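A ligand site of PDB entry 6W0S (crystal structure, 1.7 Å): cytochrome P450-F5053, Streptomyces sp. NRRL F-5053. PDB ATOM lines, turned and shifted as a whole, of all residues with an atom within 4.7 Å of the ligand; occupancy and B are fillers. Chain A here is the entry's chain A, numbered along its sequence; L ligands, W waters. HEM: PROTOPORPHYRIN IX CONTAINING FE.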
ATOM      1  N   SER A  61      28.850  11.227 -17.214  1.00  0.00           N
ATOM      2  CA  SER A  61      29.246  10.986 -15.829  1.00  0.00           C
ATOM      3  C   SER A  61      30.547  11.720 -15.514  1.00  0.00           C
ATOM      4  O   SER A  61      30.681  12.328 -14.442  1.00  0.00           O
ATOM      5  CB  SER A  61      29.419   9.497 -15.557  1.00  0.00           C
ATOM      6  OG  SER A  61      30.027   9.324 -14.276  1.00  0.00           O
ATOM      7  N   ILE A  87      38.390   5.705 -13.096  1.00  0.00           N
ATOM      8  CA  ILE A  87      37.916   4.702 -14.032  1.00  0.00           C
ATOM      9  C   ILE A  87      38.103   5.189 -15.457  1.00  0.00           C
ATOM     10  O   ILE A  87      38.516   4.428 -16.341  1.00  0.00           O
ATOM     11  CB  ILE A  87      36.470   4.301 -13.711  1.00  0.00           C
ATOM     12  CG1 ILE A  87      36.118   2.964 -14.391  1.00  0.00           C
ATOM     13  CG2 ILE A  87      35.485   5.368 -14.151  1.00  0.00           C
ATOM     14  CD1 ILE A  87      36.935   1.774 -13.925  1.00  0.00           C
ATOM     15  N   ARG A  91      40.533   3.482 -18.362  1.00  0.00           N
ATOM     16  CA  ARG A  91      40.006   3.140 -19.681  1.00  0.00           C
ATOM     17  C   ARG A  91      40.763   3.912 -20.777  1.00  0.00           C
ATOM     18  O   ARG A  91      41.023   3.373 -21.857  1.00  0.00           O
ATOM     19  CB  ARG A  91      38.493   3.420 -19.729  1.00  0.00           C
ATOM     20  CG  ARG A  91      37.642   2.370 -18.936  1.00  0.00           C
ATOM     21  CD  ARG A  91      36.143   2.733 -18.771  1.00  0.00           C
ATOM     22  NE  ARG A  91      35.381   1.693 -18.052  1.00  0.00           N
ATOM     23  CZ  ARG A  91      34.238   1.909 -17.390  1.00  0.00           C
ATOM     24  NH1 ARG A  91      33.724   3.128 -17.359  1.00  0.00           N
ATOM     25  NH2 ARG A  91      33.613   0.918 -16.759  1.00  0.00           N
ATOM     26  N   LEU A 103      37.866  -8.295 -13.284  1.00  0.00           N
ATOM     27  CA  LEU A 103      36.529  -8.186 -12.716  1.00  0.00           C
ATOM     28  C   LEU A 103      35.486  -9.067 -13.386  1.00  0.00           C
ATOM     29  O   LEU A 103      34.421  -9.280 -12.782  1.00  0.00           O
ATOM     30  CB  LEU A 103      36.028  -6.725 -12.784  1.00  0.00           C
ATOM     31  CG  LEU A 103      36.815  -5.698 -11.979  1.00  0.00           C
ATOM     32  CD1 LEU A 103      36.340  -4.281 -12.367  1.00  0.00           C
ATOM     33  CD2 LEU A 103      36.705  -5.942 -10.503  1.00  0.00           C
ATOM     34  N   LEU A 147      36.733 -10.032   0.210  1.00  0.00           N
ATOM     35  CA  LEU A 147      36.501  -9.689  -1.192  1.00  0.00           C
ATOM     36  C   LEU A 147      37.435  -8.569  -1.634  1.00  0.00           C
ATOM     37  O   LEU A 147      38.099  -8.680  -2.673  1.00  0.00           O
ATOM     38  CB  LEU A 147      35.028  -9.308  -1.387  1.00  0.00           C
ATOM     39  CG  LEU A 147      34.621  -8.743  -2.754  1.00  0.00           C
ATOM     40  CD1 LEU A 147      34.553  -9.876  -3.783  1.00  0.00           C
ATOM     41  CD2 LEU A 147      33.295  -7.969  -2.688  1.00  0.00           C
ATOM     42  N   LEU A 152      40.704  -7.219  -5.099  1.00  0.00           N
ATOM     43  CA  LEU A 152      40.932  -5.847  -5.558  1.00  0.00           C
ATOM     44  C   LEU A 152      42.314  -5.334  -5.183  1.00  0.00           C
ATOM     45  O   LEU A 152      43.086  -4.951  -6.064  1.00  0.00           O
ATOM     46  CB  LEU A 152      39.857  -4.895  -5.010  1.00  0.00           C
ATOM     47  CG  LEU A 152      38.436  -5.316  -5.353  1.00  0.00           C
ATOM     48  CD1 LEU A 152      37.409  -4.336  -4.791  1.00  0.00           C
ATOM     49  CD2 LEU A 152      38.175  -5.460  -6.834  1.00  0.00           C
ATOM     50  N   LEU A 233      39.832   4.458  -5.867  1.00  0.00           N
ATOM     51  CA  LEU A 233      38.640   4.051  -6.603  1.00  0.00           C
ATOM     52  C   LEU A 233      38.113   2.707  -6.111  1.00  0.00           C
ATOM     53  O   LEU A 233      36.919   2.546  -5.840  1.00  0.00           O
ATOM     54  CB  LEU A 233      38.952   4.004  -8.105  1.00  0.00           C
ATOM     55  CG  LEU A 233      37.883   3.300  -8.943  1.00  0.00           C
ATOM     56  CD1 LEU A 233      36.610   4.147  -8.917  1.00  0.00           C
ATOM     57  CD2 LEU A 233      38.351   3.046 -10.379  1.00  0.00           C
ATOM     58  N   LEU A 234      39.001   1.726  -5.961  1.00  0.00           N
ATOM     59  CA  LEU A 234      38.544   0.388  -5.625  1.00  0.00           C
ATOM     60  C   LEU A 234      37.984   0.318  -4.219  1.00  0.00           C
ATOM     61  O   LEU A 234      36.990  -0.382  -3.982  1.00  0.00           O
ATOM     62  CB  LEU A 234      39.677  -0.615  -5.833  1.00  0.00           C
ATOM     63  CG  LEU A 234      39.999  -0.759  -7.334  1.00  0.00           C
ATOM     64  CD1 LEU A 234      41.290  -1.588  -7.435  1.00  0.00           C
ATOM     65  CD2 LEU A 234      38.883  -1.350  -8.163  1.00  0.00           C
ATOM     66  N   ALA A 237      34.457   2.318  -4.438  1.00  0.00           N
ATOM     67  CA  ALA A 237      33.482   1.618  -5.265  1.00  0.00           C
ATOM     68  C   ALA A 237      33.114   0.265  -4.687  1.00  0.00           C
ATOM     69  O   ALA A 237      31.974  -0.199  -4.868  1.00  0.00           O
ATOM     70  CB  ALA A 237      34.036   1.427  -6.693  1.00  0.00           C
ATOM     71  N   GLY A 238      34.036  -0.379  -3.983  1.00  0.00           N
ATOM     72  CA  GLY A 238      33.859  -1.764  -3.621  1.00  0.00           C
ATOM     73  C   GLY A 238      33.574  -2.091  -2.178  1.00  0.00           C
ATOM     74  O   GLY A 238      32.910  -3.093  -1.885  1.00  0.00           O
ATOM     75  N   THR A 241      29.939  -0.276  -0.548  1.00  0.00           N
ATOM     76  CA  THR A 241      28.832  -0.798  -1.319  1.00  0.00           C
ATOM     77  C   THR A 241      28.585  -2.264  -0.965  1.00  0.00           C
ATOM     78  O   THR A 241      27.452  -2.676  -0.688  1.00  0.00           O
ATOM     79  CB  THR A 241      29.143  -0.663  -2.813  1.00  0.00           C
ATOM     80  OG1 THR A 241      30.458  -1.202  -3.011  1.00  0.00           O
ATOM     81  CG2 THR A 241      29.118   0.776  -3.282  1.00  0.00           C
ATOM     82  N   SER A 242      29.642  -3.066  -0.988  1.00  0.00           N
ATOM     83  CA  SER A 242      29.473  -4.483  -0.702  1.00  0.00           C
ATOM     84  C   SER A 242      29.029  -4.690   0.732  1.00  0.00           C
ATOM     85  O   SER A 242      28.179  -5.546   1.010  1.00  0.00           O
ATOM     86  CB  SER A 242      30.785  -5.207  -0.949  1.00  0.00           C
ATOM     87  OG  SER A 242      31.149  -5.069  -2.306  1.00  0.00           O
ATOM     88  N   PHE A 245      25.385  -3.354   1.097  1.00  0.00           N
ATOM     89  CA  PHE A 245      24.405  -4.177   0.416  1.00  0.00           C
ATOM     90  C   PHE A 245      24.236  -5.508   1.123  1.00  0.00           C
ATOM     91  O   PHE A 245      23.096  -5.997   1.271  1.00  0.00           O
ATOM     92  CB  PHE A 245      24.757  -4.444  -1.029  1.00  0.00           C
ATOM     93  CG  PHE A 245      23.631  -5.118  -1.758  1.00  0.00           C
ATOM     94  CD1 PHE A 245      22.528  -4.377  -2.152  1.00  0.00           C
ATOM     95  CD2 PHE A 245      23.602  -6.484  -1.910  1.00  0.00           C
ATOM     96  CE1 PHE A 245      21.453  -4.999  -2.769  1.00  0.00           C
ATOM     97  CE2 PHE A 245      22.527  -7.111  -2.505  1.00  0.00           C
ATOM     98  CZ  PHE A 245      21.462  -6.368  -2.946  1.00  0.00           C
ATOM     99  N   LEU A 278      18.653  -7.215  -5.423  1.00  0.00           N
ATOM    100  CA  LEU A 278      19.269  -6.038  -6.018  1.00  0.00           C
ATOM    101  C   LEU A 278      18.224  -4.983  -6.408  1.00  0.00           C
ATOM    102  O   LEU A 278      18.539  -3.789  -6.447  1.00  0.00           O
ATOM    103  CB  LEU A 278      20.106  -6.427  -7.229  1.00  0.00           C
ATOM    104  CG  LEU A 278      21.435  -7.069  -6.835  1.00  0.00           C
ATOM    105  CD1 LEU A 278      21.920  -7.984  -7.942  1.00  0.00           C
ATOM    106  CD2 LEU A 278      22.496  -6.030  -6.500  1.00  0.00           C
ATOM    107  N   LEU A 283      20.198   0.735  -1.281  1.00  0.00           N
ATOM    108  CA  LEU A 283      21.592   0.875  -0.899  1.00  0.00           C
ATOM    109  C   LEU A 283      21.958   2.342  -0.787  1.00  0.00           C
ATOM    110  O   LEU A 283      22.212   2.828   0.326  1.00  0.00           O
ATOM    111  CB  LEU A 283      22.523   0.178  -1.888  1.00  0.00           C
ATOM    112  CG  LEU A 283      23.981   0.254  -1.435  1.00  0.00           C
ATOM    113  CD1 LEU A 283      24.258  -0.386  -0.078  1.00  0.00           C
ATOM    114  CD2 LEU A 283      24.829  -0.340  -2.581  1.00  0.00           C
ATOM    115  N   VAL A 288      22.784   8.542  -8.643  1.00  0.00           N
ATOM    116  CA  VAL A 288      23.804   8.657  -9.669  1.00  0.00           C
ATOM    117  C   VAL A 288      23.581   9.980 -10.395  1.00  0.00           C
ATOM    118  O   VAL A 288      22.466  10.529 -10.417  1.00  0.00           O
ATOM    119  CB  VAL A 288      23.778   7.456 -10.633  1.00  0.00           C
ATOM    120  CG1 VAL A 288      23.993   6.169  -9.853  1.00  0.00           C
ATOM    121  CG2 VAL A 288      22.484   7.406 -11.424  1.00  0.00           C
ATOM    122  N   ARG A 290      24.633  12.810 -13.743  1.00  0.00           N
ATOM    123  CA  ARG A 290      25.149  13.072 -15.060  1.00  0.00           C
ATOM    124  C   ARG A 290      25.023  14.555 -15.373  1.00  0.00           C
ATOM    125  O   ARG A 290      24.053  15.194 -14.981  1.00  0.00           O
ATOM    126  CB  ARG A 290      24.363  12.288 -16.119  1.00  0.00           C
ATOM    127  CG  ARG A 290      24.314  10.789 -15.903  1.00  0.00           C
ATOM    128  CD  ARG A 290      25.638  10.103 -16.246  1.00  0.00           C
ATOM    129  NE  ARG A 290      25.508   8.637 -16.231  1.00  0.00           N
ATOM    130  CZ  ARG A 290      25.723   7.864 -15.171  1.00  0.00           C
ATOM    131  NH1 ARG A 290      26.074   8.400 -14.007  1.00  0.00           N
ATOM    132  NH2 ARG A 290      25.576   6.543 -15.258  1.00  0.00           N
ATOM    133  N   LEU A 313      18.352   5.436  -7.969  1.00  0.00           N
ATOM    134  CA  LEU A 313      18.155   4.044  -8.367  1.00  0.00           C
ATOM    135  C   LEU A 313      17.095   3.378  -7.499  1.00  0.00           C
ATOM    136  O   LEU A 313      16.373   2.486  -7.979  1.00  0.00           O
ATOM    137  CB  LEU A 313      19.449   3.255  -8.279  1.00  0.00           C
ATOM    138  CG  LEU A 313      20.589   3.923  -9.033  1.00  0.00           C
ATOM    139  CD1 LEU A 313      21.885   3.177  -8.649  1.00  0.00           C
ATOM    140  CD2 LEU A 313      20.442   3.973 -10.512  1.00  0.00           C
ATOM    141  N   PHE A 339      17.722  -1.628 -11.515  1.00  0.00           N
ATOM    142  CA  PHE A 339      18.723  -0.567 -11.596  1.00  0.00           C
ATOM    143  C   PHE A 339      19.744  -0.629 -10.456  1.00  0.00           C
ATOM    144  O   PHE A 339      20.448   0.360 -10.211  1.00  0.00           O
ATOM    145  CB  PHE A 339      18.024   0.805 -11.588  1.00  0.00           C
ATOM    146  CG  PHE A 339      17.672   1.337 -12.951  1.00  0.00           C
ATOM    147  CD1 PHE A 339      16.743   0.708 -13.766  1.00  0.00           C
ATOM    148  CD2 PHE A 339      18.257   2.506 -13.399  1.00  0.00           C
ATOM    149  CE1 PHE A 339      16.421   1.239 -15.010  1.00  0.00           C
ATOM    150  CE2 PHE A 339      17.934   3.030 -14.636  1.00  0.00           C
ATOM    151  CZ  PHE A 339      17.019   2.414 -15.439  1.00  0.00           C
ATOM    152  N   GLY A 340      19.850  -1.772  -9.763  1.00  0.00           N
ATOM    153  CA  GLY A 340      20.758  -1.876  -8.630  1.00  0.00           C
ATOM    154  C   GLY A 340      22.220  -1.672  -8.994  1.00  0.00           C
ATOM    155  O   GLY A 340      23.021  -1.273  -8.133  1.00  0.00           O
ATOM    156  N   PHE A 341      22.598  -1.989 -10.231  1.00  0.00           N
ATOM    157  CA  PHE A 341      23.953  -1.799 -10.746  1.00  0.00           C
ATOM    158  C   PHE A 341      24.010  -0.679 -11.768  1.00  0.00           C
ATOM    159  O   PHE A 341      25.017  -0.508 -12.477  1.00  0.00           O
ATOM    160  CB  PHE A 341      24.489  -3.076 -11.380  1.00  0.00           C
ATOM    161  CG  PHE A 341      24.808  -4.187 -10.432  1.00  0.00           C
ATOM    162  CD1 PHE A 341      25.600  -3.964  -9.314  1.00  0.00           C
ATOM    163  CD2 PHE A 341      24.338  -5.470 -10.676  1.00  0.00           C
ATOM    164  CE1 PHE A 341      25.913  -5.023  -8.441  1.00  0.00           C
ATOM    165  CE2 PHE A 341      24.631  -6.520  -9.823  1.00  0.00           C
ATOM    166  CZ  PHE A 341      25.423  -6.297  -8.705  1.00  0.00           C
ATOM    167  N   GLY A 342      22.931   0.076 -11.902  1.00  0.00           N
ATOM    168  CA  GLY A 342      22.857   1.173 -12.837  1.00  0.00           C
ATOM    169  C   GLY A 342      22.405   0.724 -14.212  1.00  0.00           C
ATOM    170  O   GLY A 342      21.651  -0.257 -14.339  1.00  0.00           O
ATOM    171  N   ARG A 345      26.348   2.360 -20.322  1.00  0.00           N
ATOM    172  CA  ARG A 345      27.799   2.218 -20.401  1.00  0.00           C
ATOM    173  C   ARG A 345      28.486   2.291 -19.040  1.00  0.00           C
ATOM    174  O   ARG A 345      29.645   1.878 -18.955  1.00  0.00           O
ATOM    175  CB  ARG A 345      28.387   3.283 -21.312  1.00  0.00           C
ATOM    176  CG  ARG A 345      28.184   4.681 -20.805  1.00  0.00           C
ATOM    177  CD  ARG A 345      28.002   5.692 -21.965  1.00  0.00           C
ATOM    178  NE  ARG A 345      27.819   7.019 -21.398  1.00  0.00           N
ATOM    179  CZ  ARG A 345      26.674   7.491 -20.941  1.00  0.00           C
ATOM    180  NH1 ARG A 345      25.575   6.752 -21.032  1.00  0.00           N
ATOM    181  NH2 ARG A 345      26.628   8.700 -20.405  1.00  0.00           N
ATOM    182  N   HIS A 346      27.843   2.832 -18.010  1.00  0.00           N
ATOM    183  CA  HIS A 346      28.422   2.888 -16.673  1.00  0.00           C
ATOM    184  C   HIS A 346      27.894   1.807 -15.731  1.00  0.00           C
ATOM    185  O   HIS A 346      28.057   1.923 -14.516  1.00  0.00           O
ATOM    186  CB  HIS A 346      28.226   4.281 -16.067  1.00  0.00           C
ATOM    187  CG  HIS A 346      28.907   5.352 -16.859  1.00  0.00           C
ATOM    188  ND1 HIS A 346      30.268   5.428 -16.975  1.00  0.00           N
ATOM    189  CD2 HIS A 346      28.403   6.345 -17.624  1.00  0.00           C
ATOM    190  CE1 HIS A 346      30.587   6.438 -17.763  1.00  0.00           C
ATOM    191  NE2 HIS A 346      29.470   7.020 -18.172  1.00  0.00           N
ATOM    192  N   CYS A 348      27.694  -1.187 -13.357  1.00  0.00           N
ATOM    193  CA  CYS A 348      28.749  -1.494 -12.415  1.00  0.00           C
ATOM    194  C   CYS A 348      29.665  -2.583 -12.922  1.00  0.00           C
ATOM    195  O   CYS A 348      29.231  -3.728 -13.089  1.00  0.00           O
ATOM    196  CB  CYS A 348      28.150  -1.911 -11.077  1.00  0.00           C
ATOM    197  SG  CYS A 348      29.372  -2.520  -9.913  1.00  0.00           S
ATOM    198  N   PRO A 349      30.951  -2.297 -13.133  1.00  0.00           N
ATOM    199  CA  PRO A 349      31.869  -3.369 -13.535  1.00  0.00           C
ATOM    200  C   PRO A 349      32.191  -4.333 -12.413  1.00  0.00           C
ATOM    201  O   PRO A 349      32.727  -5.414 -12.678  1.00  0.00           O
ATOM    202  CB  PRO A 349      33.115  -2.606 -13.993  1.00  0.00           C
ATOM    203  CG  PRO A 349      33.097  -1.351 -13.222  1.00  0.00           C
ATOM    204  CD  PRO A 349      31.643  -1.008 -12.953  1.00  0.00           C
ATOM    205  N   GLY A 350      31.915  -3.977 -11.161  1.00  0.00           N
ATOM    206  CA  GLY A 350      31.997  -4.907 -10.061  1.00  0.00           C
ATOM    207  C   GLY A 350      30.826  -5.852  -9.966  1.00  0.00           C
ATOM    208  O   GLY A 350      30.728  -6.614  -9.005  1.00  0.00           O
ATOM    209  N   ALA A 354      30.259  -8.861  -7.263  1.00  0.00           N
ATOM    210  CA  ALA A 354      29.183  -8.587  -6.312  1.00  0.00           C
ATOM    211  C   ALA A 354      28.150  -9.709  -6.323  1.00  0.00           C
ATOM    212  O   ALA A 354      27.730 -10.192  -5.268  1.00  0.00           O
ATOM    213  CB  ALA A 354      28.509  -7.254  -6.646  1.00  0.00           C
HETATM  214  CHA HEM L   1      29.623   1.774 -10.643  1.00  0.00           C
HETATM  215  CHB HEM L   1      26.550  -0.464  -7.604  1.00  0.00           C
HETATM  216  CHC HEM L   1      30.168  -3.211  -6.015  1.00  0.00           C
HETATM  217  CHD HEM L   1      33.222  -0.929  -9.021  1.00  0.00           C
HETATM  218  C1A HEM L   1      28.496   1.347  -9.987  1.00  0.00           C
HETATM  219  C2A HEM L   1      27.170   1.870 -10.272  1.00  0.00           C
HETATM  220  C3A HEM L   1      26.326   1.259  -9.415  1.00  0.00           C
HETATM  221  C4A HEM L   1      27.088   0.343  -8.575  1.00  0.00           C
HETATM  222  CMA HEM L   1      24.802   1.477  -9.308  1.00  0.00           C
HETATM  223  CAA HEM L   1      26.782   2.906 -11.379  1.00  0.00           C
HETATM  224  CBA HEM L   1      27.200   4.336 -11.020  1.00  0.00           C
HETATM  225  CGA HEM L   1      26.752   5.387 -12.030  1.00  0.00           C
HETATM  226  O1A HEM L   1      27.314   6.525 -12.039  1.00  0.00           O
HETATM  227  O2A HEM L   1      25.855   5.094 -12.839  1.00  0.00           O
HETATM  228  C1B HEM L   1      27.276  -1.396  -6.922  1.00  0.00           C
HETATM  229  C2B HEM L   1      26.737  -2.337  -5.983  1.00  0.00           C
HETATM  230  C3B HEM L   1      27.723  -3.076  -5.520  1.00  0.00           C
HETATM  231  C4B HEM L   1      28.933  -2.645  -6.177  1.00  0.00           C
HETATM  232  CMB HEM L   1      25.271  -2.397  -5.552  1.00  0.00           C
HETATM  233  CAB HEM L   1      27.597  -4.192  -4.464  1.00  0.00           C
HETATM  234  CBB HEM L   1      28.656  -4.459  -3.697  1.00  0.00           C
HETATM  235  C1C HEM L   1      31.299  -2.892  -6.720  1.00  0.00           C
HETATM  236  C2C HEM L   1      32.575  -3.558  -6.675  1.00  0.00           C
HETATM  237  C3C HEM L   1      33.380  -2.900  -7.496  1.00  0.00           C
HETATM  238  C4C HEM L   1      32.673  -1.813  -8.113  1.00  0.00           C
HETATM  239  CMC HEM L   1      32.923  -4.824  -5.838  1.00  0.00           C
HETATM  240  CAC HEM L   1      34.834  -3.214  -7.846  1.00  0.00           C
HETATM  241  CBC HEM L   1      35.317  -4.417  -7.555  1.00  0.00           C
HETATM  242  C1D HEM L   1      32.518   0.050  -9.686  1.00  0.00           C
HETATM  243  C2D HEM L   1      33.080   1.029 -10.567  1.00  0.00           C
HETATM  244  C3D HEM L   1      32.089   1.796 -11.046  1.00  0.00           C
HETATM  245  C4D HEM L   1      30.871   1.297 -10.433  1.00  0.00           C
HETATM  246  CMD HEM L   1      34.600   1.104 -10.876  1.00  0.00           C
HETATM  247  CAD HEM L   1      32.148   3.000 -12.024  1.00  0.00           C
HETATM  248  CBD HEM L   1      31.867   2.559 -13.465  1.00  0.00           C
HETATM  249  CGD HEM L   1      31.736   3.764 -14.382  1.00  0.00           C
HETATM  250  O1D HEM L   1      31.827   3.593 -15.617  1.00  0.00           O
HETATM  251  O2D HEM L   1      31.493   4.892 -13.907  1.00  0.00           O
HETATM  252  NA  HEM L   1      28.426   0.406  -8.951  1.00  0.00           N
HETATM  253  NB  HEM L   1      28.635  -1.605  -7.065  1.00  0.00           N
HETATM  254  NC  HEM L   1      31.396  -1.870  -7.623  1.00  0.00           N
HETATM  255  ND  HEM L   1      31.148   0.227  -9.597  1.00  0.00           N
HETATM  256 FE   HEM L   1      29.872  -0.798  -8.410  1.00  0.00          FE
HETATM  257  O   HOH W   1      27.148   8.846 -10.719  1.00  0.00           O
HETATM  258  O   HOH W   2      30.397   0.786  -6.862  1.00  0.00           O
HETATM  259  O   HOH W   3      32.048   7.428 -14.832  1.00  0.00           O
HETATM  260  O   HOH W   4      25.143   3.060 -14.490  1.00  0.00           O
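Water W1 lies within hydrogen-bond range of O1A of the ligand (2.7 Å) and NH1 of Arg 290 (3.5 Å). Water W4 bridges an oxygen (O2A) of the ligand (2.7 Å) and the backbone carbonyl oxygen of His 346 (3.1 Å). Water W3 lies within hydrogen-bond range of an oxygen (O2D) of the ligand (2.8 Å), the side-chain hydroxyl (OG) of Ser 61 (2.8 Å) and a ring nitrogen (ND1) of His 346 (3.4 Å).
The backbone carbonyl oxygen of Phe 341 sits at hydrogen-bond distance from the backbone NH of Cys 348. The side-chain sulfur of Cys 348 lies close to the backbone NH of Gly 350, 3.2 Å away. OG of Ser 242 sits at hydrogen-bond distance from O of Gly 238 (2.7 Å). O of Ala 237 lies within hydrogen-bond range of OG1 of Thr 241 (2.6 Å). OG1 of Thr 241 sits at hydrogen-bond distance from O of Gly 238 (3.3 Å).
An iron atom (FE) of the ligand is bound by the side-chain sulfur of Cys 348 (2.3 Å). The guanidinium group (NH1) of Arg 91 lies within salt-bridge range of an oxygen (O1D) of the ligand (2.6 Å). A ring nitrogen (ND1) of His 346 sits at hydrogen-bond distance from an oxygen (O1D) of the ligand. O2A of the ligand is in salt-bridge range of NH2 of Arg 290, at 2.8 Å.
The backbone carbonyl oxygen of Ala 237 lies close to a nitrogen (NC) of the ligand (3.3 Å). Residues that only touch the ligand: Ile 87, Leu 103, Leu 152, Gly 238, Thr 241, Ser 242, Leu 283, Val 288, Leu 313, Gly 340, Phe 341, Gly 342, Pro 349, Gly 350 and Ala 354. Hydrophobic or aromatic side chains within 4 Å of the ligand: Ile 87, Leu 103, Leu 152, Ala 237, Leu 283, Val 288, Leu 313, Phe 341, His 346, Pro 349 and Ala 354. 20 residues have an atom within 4 Å of the ligand: Ile 87, Arg 91, Leu 103, Leu 152, Ala 237, Gly 238, Thr 241, Ser 242, Leu 283, Val 288, Arg 290, Leu 313, Gly 340, Phe 341, Gly 342, His 346, Cys 348, Pro 349, Gly 350 and Ala 354. Along chain A the residues within 4 Å of the ligand span positions 87 to 354. The nearest printed residue that does not touch the ligand is Leu 233 (4.1 Å).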
